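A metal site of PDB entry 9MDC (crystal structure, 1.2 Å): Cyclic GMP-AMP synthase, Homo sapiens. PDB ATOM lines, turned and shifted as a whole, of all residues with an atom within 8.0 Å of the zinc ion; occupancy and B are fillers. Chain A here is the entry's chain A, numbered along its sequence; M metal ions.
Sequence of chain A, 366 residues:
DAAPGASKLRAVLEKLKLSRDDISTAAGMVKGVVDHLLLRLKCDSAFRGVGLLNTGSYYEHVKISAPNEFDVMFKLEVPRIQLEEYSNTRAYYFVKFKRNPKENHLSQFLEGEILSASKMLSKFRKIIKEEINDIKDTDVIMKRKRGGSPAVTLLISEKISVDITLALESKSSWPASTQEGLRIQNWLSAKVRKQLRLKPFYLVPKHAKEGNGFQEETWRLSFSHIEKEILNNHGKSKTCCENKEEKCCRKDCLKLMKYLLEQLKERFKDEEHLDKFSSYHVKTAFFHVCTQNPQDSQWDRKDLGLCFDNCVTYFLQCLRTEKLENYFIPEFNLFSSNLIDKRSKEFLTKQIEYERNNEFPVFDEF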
ATOM      1  N   LEU A 231       5.626  29.158 -30.646  1.00  0.00           N
ATOM      2  CA  LEU A 231       5.993  29.256 -29.238  1.00  0.00           C
ATOM      3  C   LEU A 231       5.033  28.480 -28.342  1.00  0.00           C
ATOM      4  O   LEU A 231       5.450  27.925 -27.326  1.00  0.00           O
ATOM      5  CB  LEU A 231       6.069  30.716 -28.795  1.00  0.00           C
ATOM      6  CG  LEU A 231       7.413  31.366 -29.148  1.00  0.00           C
ATOM      7  CD1 LEU A 231       7.352  32.863 -28.960  1.00  0.00           C
ATOM      8  CD2 LEU A 231       8.531  30.770 -28.314  1.00  0.00           C
ATOM      9  N   ASN A 233       3.363  25.752 -29.251  1.00  0.00           N
ATOM     10  CA  ASN A 233       3.365  24.349 -29.639  1.00  0.00           C
ATOM     11  C   ASN A 233       4.800  24.011 -30.034  1.00  0.00           C
ATOM     12  O   ASN A 233       5.095  23.675 -31.181  1.00  0.00           O
ATOM     13  CB  ASN A 233       2.407  24.101 -30.798  1.00  0.00           C
ATOM     14  CG  ASN A 233       0.965  24.509 -30.488  1.00  0.00           C
ATOM     15  OD1 ASN A 233       0.171  23.697 -30.010  1.00  0.00           O
ATOM     16  ND2 ASN A 233       0.605  25.753 -30.789  1.00  0.00           N
ATOM     17  N   HIS A 234       5.730  24.111 -29.080  1.00  0.00           N
ATOM     18  CA  HIS A 234       7.136  24.331 -29.380  1.00  0.00           C
ATOM     19  C   HIS A 234       8.013  23.088 -29.343  1.00  0.00           C
ATOM     20  O   HIS A 234       9.212  23.194 -29.623  1.00  0.00           O
ATOM     21  CB  HIS A 234       7.712  25.326 -28.384  1.00  0.00           C
ATOM     22  CG  HIS A 234       7.671  24.840 -26.976  1.00  0.00           C
ATOM     23  ND1 HIS A 234       6.885  25.417 -26.002  1.00  0.00           N
ATOM     24  CD2 HIS A 234       8.279  23.779 -26.376  1.00  0.00           C
ATOM     25  CE1 HIS A 234       7.020  24.758 -24.872  1.00  0.00           C
ATOM     26  NE2 HIS A 234       7.864  23.756 -25.060  1.00  0.00           N
ATOM     27  N   GLY A 235       7.469  21.919 -28.964  1.00  0.00           N
ATOM     28  CA  GLY A 235       8.307  20.746 -28.822  1.00  0.00           C
ATOM     29  C   GLY A 235       8.332  19.879 -30.062  1.00  0.00           C
ATOM     30  O   GLY A 235       7.428  19.928 -30.895  1.00  0.00           O
ATOM     31  N   LYS A 236       9.380  19.074 -30.206  1.00  0.00           N
ATOM     32  CA  LYS A 236       9.277  17.966 -31.140  1.00  0.00           C
ATOM     33  C   LYS A 236       8.204  16.995 -30.667  1.00  0.00           C
ATOM     34  O   LYS A 236       7.384  16.517 -31.466  1.00  0.00           O
ATOM     35  CB  LYS A 236      10.625  17.252 -31.303  1.00  0.00           C
ATOM     36  CG  LYS A 236      10.500  15.983 -32.144  1.00  0.00           C
ATOM     37  CD  LYS A 236      11.856  15.342 -32.415  1.00  0.00           C
ATOM     38  CE  LYS A 236      12.726  16.204 -33.330  1.00  0.00           C
ATOM     39  NZ  LYS A 236      12.017  16.549 -34.608  1.00  0.00           N
ATOM     40  N   SER A 237       8.184  16.704 -29.376  1.00  0.00           N
ATOM     41  CA  SER A 237       7.092  15.926 -28.793  1.00  0.00           C
ATOM     42  C   SER A 237       5.863  16.794 -28.661  1.00  0.00           C
ATOM     43  O   SER A 237       5.944  17.922 -28.152  1.00  0.00           O
ATOM     44  CB  SER A 237       7.478  15.441 -27.404  1.00  0.00           C
ATOM     45  OG  SER A 237       6.333  14.828 -26.828  1.00  0.00           O
ATOM     46  N   THR A 239       3.671  16.368 -26.513  1.00  0.00           N
ATOM     47  CA  THR A 239       3.424  16.521 -25.094  1.00  0.00           C
ATOM     48  C   THR A 239       4.548  17.277 -24.368  1.00  0.00           C
ATOM     49  O   THR A 239       4.568  17.285 -23.140  1.00  0.00           O
ATOM     50  CB  THR A 239       3.096  15.175 -24.419  1.00  0.00           C
ATOM     51  OG1 THR A 239       4.051  14.173 -24.814  1.00  0.00           O
ATOM     52  CG2 THR A 239       1.680  14.710 -24.825  1.00  0.00           C
ATOM     53  N   CYS A 240       5.443  17.940 -25.111  1.00  0.00           N
ATOM     54  CA  CYS A 240       6.445  18.776 -24.449  1.00  0.00           C
ATOM     55  C   CYS A 240       5.748  19.754 -23.518  1.00  0.00           C
ATOM     56  O   CYS A 240       4.779  20.414 -23.897  1.00  0.00           O
ATOM     57  CB  CYS A 240       7.285  19.535 -25.491  1.00  0.00           C
ATOM     58  SG  CYS A 240       8.828  20.263 -24.850  1.00  0.00           S
ATOM     59  N   CYS A 241       6.245  19.835 -22.280  1.00  0.00           N
ATOM     60  CA  CYS A 241       5.740  20.732 -21.240  1.00  0.00           C
ATOM     61  C   CYS A 241       4.332  20.410 -20.763  1.00  0.00           C
ATOM     62  O   CYS A 241       3.735  21.208 -20.016  1.00  0.00           O
ATOM     63  CB  CYS A 241       5.921  22.211 -21.597  1.00  0.00           C
ATOM     64  SG  CYS A 241       7.674  22.705 -21.695  1.00  0.00           S
ATOM     65  N   GLU A 242       3.777  19.245 -21.124  1.00  0.00           N
ATOM     66  CA  GLU A 242       2.488  18.803 -20.604  1.00  0.00           C
ATOM     67  C   GLU A 242       2.599  17.829 -19.434  1.00  0.00           C
ATOM     68  O   GLU A 242       1.567  17.444 -18.879  1.00  0.00           O
ATOM     69  CB  GLU A 242       1.630  18.178 -21.707  1.00  0.00           C
ATOM     70  CG  GLU A 242       1.112  19.179 -22.741  1.00  0.00           C
ATOM     71  CD  GLU A 242      -0.074  18.665 -23.551  1.00  0.00           C
ATOM     72  OE1 GLU A 242      -0.454  17.472 -23.429  1.00  0.00           O
ATOM     73  OE2 GLU A 242      -0.628  19.477 -24.318  1.00  0.00           O
ATOM     74  N   ASN A 243       3.808  17.406 -19.069  1.00  0.00           N
ATOM     75  CA  ASN A 243       3.986  16.513 -17.935  1.00  0.00           C
ATOM     76  C   ASN A 243       5.365  16.750 -17.331  1.00  0.00           C
ATOM     77  O   ASN A 243       6.218  17.408 -17.942  1.00  0.00           O
ATOM     78  CB  ASN A 243       3.795  15.044 -18.335  1.00  0.00           C
ATOM     79  CG  ASN A 243       4.796  14.587 -19.380  1.00  0.00           C
ATOM     80  OD1 ASN A 243       5.976  14.436 -19.091  1.00  0.00           O
ATOM     81  ND2 ASN A 243       4.313  14.373 -20.600  1.00  0.00           N
ATOM     82  N   GLU A 246       8.589  15.952 -19.308  1.00  0.00           N
ATOM     83  CA  GLU A 246       8.862  16.654 -20.559  1.00  0.00           C
ATOM     84  C   GLU A 246       8.906  18.163 -20.370  1.00  0.00           C
ATOM     85  O   GLU A 246       8.518  18.927 -21.269  1.00  0.00           O
ATOM     86  CB  GLU A 246       7.852  16.267 -21.643  1.00  0.00           C
ATOM     87  CG  GLU A 246       7.922  14.823 -22.058  1.00  0.00           C
ATOM     88  CD  GLU A 246       7.010  14.509 -23.216  1.00  0.00           C
ATOM     89  OE1 GLU A 246       7.315  14.954 -24.330  1.00  0.00           O
ATOM     90  OE2 GLU A 246       5.973  13.842 -23.004  1.00  0.00           O
ATOM     91  N   LYS A 247       9.389  18.634 -19.225  1.00  0.00           N
ATOM     92  CA  LYS A 247       9.499  20.071 -18.982  1.00  0.00           C
ATOM     93  C   LYS A 247      10.802  20.574 -19.590  1.00  0.00           C
ATOM     94  O   LYS A 247      11.878  20.393 -19.025  1.00  0.00           O
ATOM     95  CB  LYS A 247       9.444  20.369 -17.496  1.00  0.00           C
ATOM     96  CG  LYS A 247       8.194  19.851 -16.813  1.00  0.00           C
ATOM     97  CD  LYS A 247       6.935  20.512 -17.354  1.00  0.00           C
ATOM     98  CE  LYS A 247       6.882  21.988 -17.019  1.00  0.00           C
ATOM     99  NZ  LYS A 247       5.562  22.577 -17.385  1.00  0.00           N
ATOM    100  N   CYS A 248      10.713  21.220 -20.743  1.00  0.00           N
ATOM    101  CA  CYS A 248      11.902  21.750 -21.380  1.00  0.00           C
ATOM    102  C   CYS A 248      12.156  23.175 -20.884  1.00  0.00           C
ATOM    103  O   CYS A 248      11.327  23.786 -20.215  1.00  0.00           O
ATOM    104  CB  CYS A 248      11.787  21.696 -22.900  1.00  0.00           C
ATOM    105  SG  CYS A 248      10.794  23.023 -23.680  1.00  0.00           S
ATOM    106  N   CYS A 249      13.310  23.715 -21.265  1.00  0.00           N
ATOM    107  CA  CYS A 249      13.708  25.058 -20.834  1.00  0.00           C
ATOM    108  C   CYS A 249      13.706  26.073 -21.973  1.00  0.00           C
ATOM    109  O   CYS A 249      14.286  27.147 -21.837  1.00  0.00           O
ATOM    110  CB  CYS A 249      15.040  25.034 -20.084  1.00  0.00           C
ATOM    111  SG  CYS A 249      16.470  24.606 -21.095  1.00  0.00           S
ATOM    112  N   ARG A 250      13.017  25.779 -23.086  1.00  0.00           N
ATOM    113  CA  ARG A 250      13.020  26.714 -24.219  1.00  0.00           C
ATOM    114  C   ARG A 250      12.494  28.087 -23.801  1.00  0.00           C
ATOM    115  O   ARG A 250      13.159  29.110 -24.010  1.00  0.00           O
ATOM    116  CB  ARG A 250      12.197  26.157 -25.387  1.00  0.00           C
ATOM    117  CG  ARG A 250      12.838  25.014 -26.129  1.00  0.00           C
ATOM    118  CD  ARG A 250      11.977  24.606 -27.328  1.00  0.00           C
ATOM    119  NE  ARG A 250      12.533  23.504 -28.106  1.00  0.00           N
ATOM    120  CZ  ARG A 250      12.205  22.227 -27.923  1.00  0.00           C
ATOM    121  NH1 ARG A 250      11.460  21.851 -26.887  1.00  0.00           N
ATOM    122  NH2 ARG A 250      12.583  21.330 -28.819  1.00  0.00           N
ATOM    123  N   LYS A 251      11.290  28.141 -23.243  1.00  0.00           N
ATOM    124  CA  LYS A 251      10.724  29.444 -22.938  1.00  0.00           C
ATOM    125  C   LYS A 251      11.506  30.150 -21.838  1.00  0.00           C
ATOM    126  O   LYS A 251      11.623  31.374 -21.849  1.00  0.00           O
ATOM    127  CB  LYS A 251       9.244  29.328 -22.571  1.00  0.00           C
ATOM    128  CG  LYS A 251       8.377  29.012 -23.759  1.00  0.00           C
ATOM    129  CD  LYS A 251       6.897  29.238 -23.452  1.00  0.00           C
ATOM    130  CE  LYS A 251       6.132  29.180 -24.744  1.00  0.00           C
ATOM    131  NZ  LYS A 251       4.686  29.337 -24.579  1.00  0.00           N
ATOM    132  N   ASP A 296      13.931  17.749 -28.113  1.00  0.00           N
ATOM    133  CA  ASP A 296      13.561  18.190 -26.779  1.00  0.00           C
ATOM    134  C   ASP A 296      14.630  17.865 -25.756  1.00  0.00           C
ATOM    135  O   ASP A 296      14.812  18.613 -24.779  1.00  0.00           O
ATOM    136  CB  ASP A 296      12.225  17.585 -26.360  1.00  0.00           C
ATOM    137  CG  ASP A 296      11.066  17.989 -27.250  1.00  0.00           C
ATOM    138  OD1 ASP A 296      11.155  19.007 -27.959  1.00  0.00           O
ATOM    139  OD2 ASP A 296      10.042  17.287 -27.242  1.00  0.00           O
ATOM    140  N   TRP A 299      17.053  20.495 -24.612  1.00  0.00           N
ATOM    141  CA  TRP A 299      16.464  21.571 -23.833  1.00  0.00           C
ATOM    142  C   TRP A 299      15.954  21.048 -22.494  1.00  0.00           C
ATOM    143  O   TRP A 299      14.944  21.516 -21.977  1.00  0.00           O
ATOM    144  CB  TRP A 299      15.345  22.258 -24.619  1.00  0.00           C
ATOM    145  CG  TRP A 299      15.773  22.890 -25.894  1.00  0.00           C
ATOM    146  CD1 TRP A 299      15.798  22.324 -27.130  1.00  0.00           C
ATOM    147  CD2 TRP A 299      16.237  24.234 -26.060  1.00  0.00           C
ATOM    148  NE1 TRP A 299      16.240  23.226 -28.065  1.00  0.00           N
ATOM    149  CE2 TRP A 299      16.517  24.406 -27.427  1.00  0.00           C
ATOM    150  CE3 TRP A 299      16.438  25.304 -25.175  1.00  0.00           C
ATOM    151  CZ2 TRP A 299      16.958  25.623 -27.946  1.00  0.00           C
ATOM    152  CZ3 TRP A 299      16.880  26.516 -25.702  1.00  0.00           C
ATOM    153  CH2 TRP A 299      17.155  26.659 -27.074  1.00  0.00           C
HETATM  154 ZN    ZN M   1       8.563  22.299 -23.787  1.00  0.00          ZN
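A ring nitrogen (ND1) of His 234 lies within hydrogen-bond range of the backbone carbonyl oxygen of Leu 231.
The backbone carbonyl oxygen (O) of Glu 246 is in hydrogen-bond range of the backbone NH (N) of Cys 241 (2.6 Å).
The backbone carbonyl oxygen of Cys 241 sits at hydrogen-bond distance from the side-chain amino group of Lys 247 (3.5 Å).
The guanidinium group (NH1) of Arg 250 lies close to the side-chain sulfur (SG) of Cys 248 (3.5 Å).
NH1 of Arg 250 lies close to SG of Cys 240 (3.7 Å).
Within 4 Å of the zinc ion: His 234, Cys 240, Cys 241 and Cys 248.
The zinc ion is bound by a ring nitrogen (NE2) of His 234, the side-chain sulfur (SG) of Cys 241, the side-chain sulfur (SG) of Cys 240 and the side-chain sulfur (SG) of Cys 248.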
